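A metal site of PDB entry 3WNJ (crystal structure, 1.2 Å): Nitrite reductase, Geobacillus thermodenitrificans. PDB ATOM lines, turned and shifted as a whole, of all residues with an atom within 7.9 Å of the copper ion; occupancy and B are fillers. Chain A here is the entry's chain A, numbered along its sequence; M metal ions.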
ATOM      1  N   ALA A  47      12.116  -1.324  15.132  1.00  0.00           N
ATOM      2  CA  ALA A  47      13.347  -0.867  15.812  1.00  0.00           C
ATOM      3  C   ALA A  47      12.890  -0.311  17.175  1.00  0.00           C
ATOM      4  O   ALA A  47      11.941   0.488  17.241  1.00  0.00           O
ATOM      5  CB  ALA A  47      13.999   0.236  15.013  1.00  0.00           C
ATOM      6  N   TRP A  63      19.812  -1.029  21.473  1.00  0.00           N
ATOM      7  CA  TRP A  63      19.064  -0.693  20.247  1.00  0.00           C
ATOM      8  C   TRP A  63      18.819  -2.006  19.529  1.00  0.00           C
ATOM      9  O   TRP A  63      19.765  -2.744  19.296  1.00  0.00           O
ATOM     10  CB  TRP A  63      19.900   0.226  19.356  1.00  0.00           C
ATOM     11  CG  TRP A  63      20.290   1.519  20.007  1.00  0.00           C
ATOM     12  CD1 TRP A  63      20.172   1.958  21.339  1.00  0.00           C
ATOM     13  CD2 TRP A  63      20.961   2.603  19.332  1.00  0.00           C
ATOM     14  NE1 TRP A  63      20.684   3.223  21.436  1.00  0.00           N
ATOM     15  CE2 TRP A  63      21.190   3.661  20.264  1.00  0.00           C
ATOM     16  CE3 TRP A  63      21.425   2.706  17.982  1.00  0.00           C
ATOM     17  CZ2 TRP A  63      21.854   4.827  19.906  1.00  0.00           C
ATOM     18  CZ3 TRP A  63      22.114   3.883  17.634  1.00  0.00           C
ATOM     19  CH2 TRP A  63      22.294   4.933  18.574  1.00  0.00           C
ATOM     20  N   THR A  64      17.542  -2.333  19.216  1.00  0.00           N
ATOM     21  CA  THR A  64      17.211  -3.667  18.795  1.00  0.00           C
ATOM     22  C   THR A  64      16.222  -3.619  17.685  1.00  0.00           C
ATOM     23  O   THR A  64      15.466  -2.669  17.441  1.00  0.00           O
ATOM     24  CB  THR A  64      16.535  -4.485  19.909  1.00  0.00           C
ATOM     25  OG1 THR A  64      15.198  -4.056  20.153  1.00  0.00           O
ATOM     26  CG2 THR A  64      17.317  -4.411  21.231  1.00  0.00           C
ATOM     27  N   PHE A  65      16.182  -4.778  16.973  1.00  0.00           N
ATOM     28  CA  PHE A  65      14.978  -5.199  16.223  1.00  0.00           C
ATOM     29  C   PHE A  65      14.111  -6.041  17.121  1.00  0.00           C
ATOM     30  O   PHE A  65      14.559  -7.050  17.692  1.00  0.00           O
ATOM     31  CB  PHE A  65      15.412  -5.998  15.009  1.00  0.00           C
ATOM     32  CG  PHE A  65      16.198  -5.157  14.050  1.00  0.00           C
ATOM     33  CD1 PHE A  65      15.565  -4.142  13.235  1.00  0.00           C
ATOM     34  CD2 PHE A  65      17.593  -5.334  13.918  1.00  0.00           C
ATOM     35  CE1 PHE A  65      16.328  -3.455  12.329  1.00  0.00           C
ATOM     36  CE2 PHE A  65      18.330  -4.595  12.971  1.00  0.00           C
ATOM     37  CZ  PHE A  65      17.687  -3.646  12.165  1.00  0.00           C
ATOM     38  N   LEU A  86       9.794  -1.863   8.334  1.00  0.00           N
ATOM     39  CA  LEU A  86      10.376  -1.491   9.606  1.00  0.00           C
ATOM     40  C   LEU A  86       9.513  -0.409  10.236  1.00  0.00           C
ATOM     41  O   LEU A  86       9.288   0.614   9.629  1.00  0.00           O
ATOM     42  CB  LEU A  86      11.804  -0.973   9.418  1.00  0.00           C
ATOM     43  CG  LEU A  86      12.535  -0.649  10.746  1.00  0.00           C
ATOM     44  CD1 LEU A  86      12.742  -1.872  11.600  1.00  0.00           C
ATOM     45  CD2 LEU A  86      13.860   0.037  10.417  1.00  0.00           C
ATOM     46  N   ASN A  88       9.664   2.098  13.196  1.00  0.00           N
ATOM     47  CA  ASN A  88      10.673   2.630  14.109  1.00  0.00           C
ATOM     48  C   ASN A  88      10.019   3.194  15.397  1.00  0.00           C
ATOM     49  O   ASN A  88       9.327   4.219  15.344  1.00  0.00           O
ATOM     50  CB  ASN A  88      11.464   3.736  13.448  1.00  0.00           C
ATOM     51  CG  ASN A  88      12.637   4.169  14.293  1.00  0.00           C
ATOM     52  OD1 ASN A  88      12.821   3.669  15.418  1.00  0.00           O
ATOM     53  ND2 ASN A  88      13.408   5.171  13.819  1.00  0.00           N
ATOM     54  N   ASP A  90      11.816   3.865  18.116  1.00  0.00           N
ATOM     55  CA  ASP A  90      12.735   4.716  18.843  1.00  0.00           C
ATOM     56  C   ASP A  90      12.233   6.136  18.828  1.00  0.00           C
ATOM     57  O   ASP A  90      11.887   6.648  17.782  1.00  0.00           O
ATOM     58  CB  ASP A  90      14.084   4.612  18.096  1.00  0.00           C
ATOM     59  CG  ASP A  90      15.230   5.233  18.817  1.00  0.00           C
ATOM     60  OD1 ASP A  90      15.063   6.382  19.389  1.00  0.00           O
ATOM     61  OD2 ASP A  90      16.345   4.722  18.840  1.00  0.00           O
ATOM     62  N   VAL A  93      16.007   8.289  17.392  1.00  0.00           N
ATOM     63  CA  VAL A  93      17.065   7.951  16.432  1.00  0.00           C
ATOM     64  C   VAL A  93      16.443   7.261  15.245  1.00  0.00           C
ATOM     65  O   VAL A  93      15.625   6.320  15.397  1.00  0.00           O
ATOM     66  CB  VAL A  93      18.082   6.995  17.094  1.00  0.00           C
ATOM     67  CG1 VAL A  93      19.276   6.772  16.182  1.00  0.00           C
ATOM     68  CG2 VAL A  93      18.588   7.573  18.406  1.00  0.00           C
ATOM     69  N   PRO A  94      16.814   7.647  13.994  1.00  0.00           N
ATOM     70  CA  PRO A  94      16.340   6.895  12.821  1.00  0.00           C
ATOM     71  C   PRO A  94      17.017   5.519  12.841  1.00  0.00           C
ATOM     72  O   PRO A  94      18.139   5.329  13.331  1.00  0.00           O
ATOM     73  CB  PRO A  94      16.872   7.750  11.659  1.00  0.00           C
ATOM     74  CG  PRO A  94      17.169   9.135  12.252  1.00  0.00           C
ATOM     75  CD  PRO A  94      17.679   8.789  13.627  1.00  0.00           C
ATOM     76  N   HIS A  95      16.406   4.540  12.115  1.00  0.00           N
ATOM     77  CA  HIS A  95      16.974   3.218  11.992  1.00  0.00           C
ATOM     78  C   HIS A  95      16.612   2.708  10.588  1.00  0.00           C
ATOM     79  O   HIS A  95      15.772   3.263   9.871  1.00  0.00           O
ATOM     80  CB  HIS A  95      16.391   2.265  13.022  1.00  0.00           C
ATOM     81  CG  HIS A  95      16.822   2.634  14.411  1.00  0.00           C
ATOM     82  ND1 HIS A  95      18.170   2.574  14.839  1.00  0.00           N
ATOM     83  CD2 HIS A  95      16.119   3.179  15.437  1.00  0.00           C
ATOM     84  CE1 HIS A  95      18.220   3.023  16.042  1.00  0.00           C
ATOM     85  NE2 HIS A  95      16.977   3.397  16.464  1.00  0.00           N
ATOM     86  N   SER A  96      17.266   1.632  10.196  1.00  0.00           N
ATOM     87  CA  SER A  96      17.102   1.084   8.840  1.00  0.00           C
ATOM     88  C   SER A  96      17.382  -0.420   8.887  1.00  0.00           C
ATOM     89  O   SER A  96      17.700  -0.952   9.987  1.00  0.00           O
ATOM     90  CB  SER A  96      18.081   1.789   7.882  1.00  0.00           C
ATOM     91  OG  SER A  96      19.410   1.621   8.319  1.00  0.00           O
ATOM     92  N   MET A  97      17.309  -1.070   7.738  1.00  0.00           N
ATOM     93  CA  MET A  97      17.620  -2.500   7.651  1.00  0.00           C
ATOM     94  C   MET A  97      18.400  -2.827   6.413  1.00  0.00           C
ATOM     95  O   MET A  97      18.024  -2.425   5.296  1.00  0.00           O
ATOM     96  CB  MET A  97      16.302  -3.291   7.656  1.00  0.00           C
ATOM     97  CG  MET A  97      16.461  -4.794   7.388  1.00  0.00           C
ATOM     98  SD  MET A  97      17.432  -5.648   8.625  1.00  0.00           S
ATOM     99  CE  MET A  97      16.109  -5.965   9.839  1.00  0.00           C
ATOM    100  N   ASP A 112      16.849   5.200   5.864  1.00  0.00           N
ATOM    101  CA  ASP A 112      16.356   5.445   7.234  1.00  0.00           C
ATOM    102  C   ASP A 112      14.869   5.573   7.313  1.00  0.00           C
ATOM    103  O   ASP A 112      14.226   6.135   6.407  1.00  0.00           O
ATOM    104  CB  ASP A 112      16.980   6.733   7.794  1.00  0.00           C
ATOM    105  CG  ASP A 112      18.460   6.514   8.095  1.00  0.00           C
ATOM    106  OD1 ASP A 112      19.002   5.412   8.095  1.00  0.00           O
ATOM    107  OD2 ASP A 112      19.146   7.558   8.193  1.00  0.00           O
ATOM    108  N   VAL A 113      14.324   5.070   8.390  1.00  0.00           N
ATOM    109  CA  VAL A 113      12.940   5.252   8.780  1.00  0.00           C
ATOM    110  C   VAL A 113      13.008   6.136  10.033  1.00  0.00           C
ATOM    111  O   VAL A 113      13.681   5.778  11.008  1.00  0.00           O
ATOM    112  CB  VAL A 113      12.287   3.896   9.060  1.00  0.00           C
ATOM    113  CG1 VAL A 113      10.862   4.094   9.630  1.00  0.00           C
ATOM    114  CG2 VAL A 113      12.305   2.994   7.840  1.00  0.00           C
ATOM    115  N   HIS A 134      21.375  -6.234   9.662  1.00  0.00           N
ATOM    116  CA  HIS A 134      21.709  -5.234  10.674  1.00  0.00           C
ATOM    117  C   HIS A 134      21.135  -3.904  10.247  1.00  0.00           C
ATOM    118  O   HIS A 134      20.832  -3.644   9.087  1.00  0.00           O
ATOM    119  CB  HIS A 134      23.219  -5.137  10.867  1.00  0.00           C
ATOM    120  CG  HIS A 134      23.980  -4.776   9.609  1.00  0.00           C
ATOM    121  ND1 HIS A 134      24.200  -3.450   9.218  1.00  0.00           N
ATOM    122  CD2 HIS A 134      24.639  -5.570   8.701  1.00  0.00           C
ATOM    123  CE1 HIS A 134      24.992  -3.512   8.065  1.00  0.00           C
ATOM    124  NE2 HIS A 134      25.233  -4.756   7.755  1.00  0.00           N
ATOM    125  N   CYS A 135      21.060  -2.979  11.238  1.00  0.00           N
ATOM    126  CA  CYS A 135      20.739  -1.605  10.892  1.00  0.00           C
ATOM    127  C   CYS A 135      21.846  -0.994  10.053  1.00  0.00           C
ATOM    128  O   CYS A 135      23.019  -1.264  10.310  1.00  0.00           O
ATOM    129  CB  CYS A 135      20.532  -0.860  12.215  1.00  0.00           C
ATOM    130  SG  CYS A 135      20.096   0.887  11.876  1.00  0.00           S
ATOM    131  N   GLY A 136      21.459  -0.175   9.055  1.00  0.00           N
ATOM    132  CA  GLY A 136      22.402   0.482   8.194  1.00  0.00           C
ATOM    133  C   GLY A 136      22.462   1.926   8.299  1.00  0.00           C
ATOM    134  O   GLY A 136      22.900   2.578   7.368  1.00  0.00           O
ATOM    135  N   THR A 137      22.099   2.482   9.467  1.00  0.00           N
ATOM    136  CA  THR A 137      22.085   3.935   9.656  1.00  0.00           C
ATOM    137  C   THR A 137      23.445   4.446  10.151  1.00  0.00           C
ATOM    138  O   THR A 137      24.074   3.814  11.001  1.00  0.00           O
ATOM    139  CB  THR A 137      20.964   4.254  10.680  1.00  0.00           C
ATOM    140  OG1 THR A 137      19.707   3.813  10.160  1.00  0.00           O
ATOM    141  CG2 THR A 137      20.897   5.713  11.018  1.00  0.00           C
ATOM    142  N   LYS A 138      23.884   5.549   9.596  1.00  0.00           N
ATOM    143  CA  LYS A 138      25.200   6.091   9.962  1.00  0.00           C
ATOM    144  C   LYS A 138      25.200   6.660  11.361  1.00  0.00           C
ATOM    145  O   LYS A 138      24.200   7.359  11.688  1.00  0.00           O
ATOM    146  CB  LYS A 138      25.551   7.222   8.946  1.00  0.00           C
ATOM    147  CG  LYS A 138      26.899   7.814   9.172  1.00  0.00           C
ATOM    148  CD  LYS A 138      27.214   8.953   8.201  1.00  0.00           C
ATOM    149  CE  LYS A 138      28.670   9.373   8.348  1.00  0.00           C
ATOM    150  NZ  LYS A 138      28.973  10.546   7.502  1.00  0.00           N
ATOM    151  N   PRO A 139      26.195   6.421  12.186  1.00  0.00           N
ATOM    152  CA  PRO A 139      27.338   5.559  11.955  1.00  0.00           C
ATOM    153  C   PRO A 139      26.953   4.118  12.194  1.00  0.00           C
ATOM    154  O   PRO A 139      26.405   3.741  13.236  1.00  0.00           O
ATOM    155  CB  PRO A 139      28.342   5.972  13.064  1.00  0.00           C
ATOM    156  CG  PRO A 139      27.737   7.127  13.760  1.00  0.00           C
ATOM    157  CD  PRO A 139      26.247   7.116  13.480  1.00  0.00           C
ATOM    158  N   VAL A 140      27.169   3.292  11.167  1.00  0.00           N
ATOM    159  CA  VAL A 140      26.708   1.905  11.251  1.00  0.00           C
ATOM    160  C   VAL A 140      27.351   1.182  12.406  1.00  0.00           C
ATOM    161  O   VAL A 140      26.711   0.373  13.068  1.00  0.00           O
ATOM    162  CB  VAL A 140      26.970   1.174   9.899  1.00  0.00           C
ATOM    163  CG1 VAL A 140      26.619  -0.303  10.008  1.00  0.00           C
ATOM    164  CG2 VAL A 140      26.094   1.840   8.780  1.00  0.00           C
ATOM    165  N   GLN A 142      27.906   2.248  15.290  1.00  0.00           N
ATOM    166  CA  GLN A 142      27.120   2.562  16.528  1.00  0.00           C
ATOM    167  C   GLN A 142      25.848   1.717  16.584  1.00  0.00           C
ATOM    168  O   GLN A 142      25.483   1.201  17.605  1.00  0.00           O
ATOM    169  CB  GLN A 142      26.785   4.045  16.489  1.00  0.00           C
ATOM    170  CG  GLN A 142      26.121   4.497  17.787  1.00  0.00           C
ATOM    171  CD  GLN A 142      25.937   5.977  17.847  1.00  0.00           C
ATOM    172  OE1 GLN A 142      26.020   6.678  16.833  1.00  0.00           O
ATOM    173  NE2 GLN A 142      25.630   6.453  18.989  1.00  0.00           N
ATOM    174  N   HIS A 143      25.150   1.655  15.422  1.00  0.00           N
ATOM    175  CA  HIS A 143      23.857   0.907  15.393  1.00  0.00           C
ATOM    176  C   HIS A 143      24.123  -0.540  15.643  1.00  0.00           C
ATOM    177  O   HIS A 143      23.372  -1.206  16.385  1.00  0.00           O
ATOM    178  CB  HIS A 143      23.146   1.257  14.186  1.00  0.00           C
ATOM    179  CG  HIS A 143      22.613   2.660  14.182  1.00  0.00           C
ATOM    180  ND1 HIS A 143      21.275   2.927  14.368  1.00  0.00           N
ATOM    181  CD2 HIS A 143      23.224   3.876  14.044  1.00  0.00           C
ATOM    182  CE1 HIS A 143      21.092   4.238  14.334  1.00  0.00           C
ATOM    183  NE2 HIS A 143      22.246   4.836  14.136  1.00  0.00           N
ATOM    184  N   ILE A 144      25.122  -1.137  14.955  1.00  0.00           N
ATOM    185  CA  ILE A 144      25.387  -2.553  15.161  1.00  0.00           C
ATOM    186  C   ILE A 144      25.853  -2.817  16.570  1.00  0.00           C
ATOM    187  O   ILE A 144      25.335  -3.683  17.278  1.00  0.00           O
ATOM    188  CB  ILE A 144      26.454  -3.097  14.167  1.00  0.00           C
ATOM    189  CG1 ILE A 144      25.938  -2.956  12.706  1.00  0.00           C
ATOM    190  CG2 ILE A 144      26.815  -4.521  14.534  1.00  0.00           C
ATOM    191  CD1 ILE A 144      26.972  -3.414  11.683  1.00  0.00           C
ATOM    192  N   ASN A 146      25.329  -1.262  19.343  1.00  0.00           N
ATOM    193  CA  ASN A 146      24.266  -1.124  20.296  1.00  0.00           C
ATOM    194  C   ASN A 146      23.229  -2.241  20.313  1.00  0.00           C
ATOM    195  O   ASN A 146      22.366  -2.287  21.140  1.00  0.00           O
ATOM    196  CB  ASN A 146      23.587   0.200  20.198  1.00  0.00           C
ATOM    197  CG  ASN A 146      24.373   1.325  20.877  1.00  0.00           C
ATOM    198  OD1 ASN A 146      25.060   1.100  21.877  1.00  0.00           O
ATOM    199  ND2 ASN A 146      24.290   2.530  20.338  1.00  0.00           N
ATOM    200  N   GLY A 147      23.315  -3.132  19.286  1.00  0.00           N
ATOM    201  CA  GLY A 147      22.480  -4.373  19.261  1.00  0.00           C
ATOM    202  C   GLY A 147      21.707  -4.632  17.982  1.00  0.00           C
ATOM    203  O   GLY A 147      21.032  -5.675  17.964  1.00  0.00           O
ATOM    204  N   MET A 148      21.841  -3.829  16.944  1.00  0.00           N
ATOM    205  CA  MET A 148      20.959  -3.963  15.818  1.00  0.00           C
ATOM    206  C   MET A 148      21.608  -4.927  14.736  1.00  0.00           C
ATOM    207  O   MET A 148      22.068  -4.455  13.686  1.00  0.00           O
ATOM    208  CB  MET A 148      20.650  -2.597  15.209  1.00  0.00           C
ATOM    209  CG  MET A 148      20.023  -1.738  16.340  1.00  0.00           C
ATOM    210  SD  MET A 148      19.208  -0.220  15.641  1.00  0.00           S
ATOM    211  CE  MET A 148      17.707  -0.967  15.044  1.00  0.00           C
HETATM  212 CU    CU M   1      19.696   1.644  13.888  1.00  0.00          CU
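The backbone carbonyl oxygen (O) of Val 93 lies close to a ring nitrogen (NE2) of His 95. A ring nitrogen (NE2) of His 95 is in hydrogen-bond range of the side-chain carboxylate (OD2) of Asp 90, 2.8 Å away. O of His 95 lies within hydrogen-bond range of N of Val 113, at 2.7 Å. The side-chain sulfur of Cys 135 lies close to the side-chain hydroxyl of Thr 137 (3.4 Å). SG of Cys 135 lies close to N of Ser 96, 3.4 Å away. O of Trp 63 lies close to N of Met 148, at 3.3 Å.
Within 4 Å of the copper ion: His 95, Cys 135, His 143 and Met 148.
The copper ion is bound by a ring nitrogen (ND1) of His 95 (2.0 Å), a ring nitrogen (ND1) of His 143 (2.1 Å), the side-chain sulfur (SG) of Cys 135 (2.2 Å) and the side-chain sulfur (SD) of Met 148 (2.6 Å). The copper ion has four donor atoms within binding distance.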
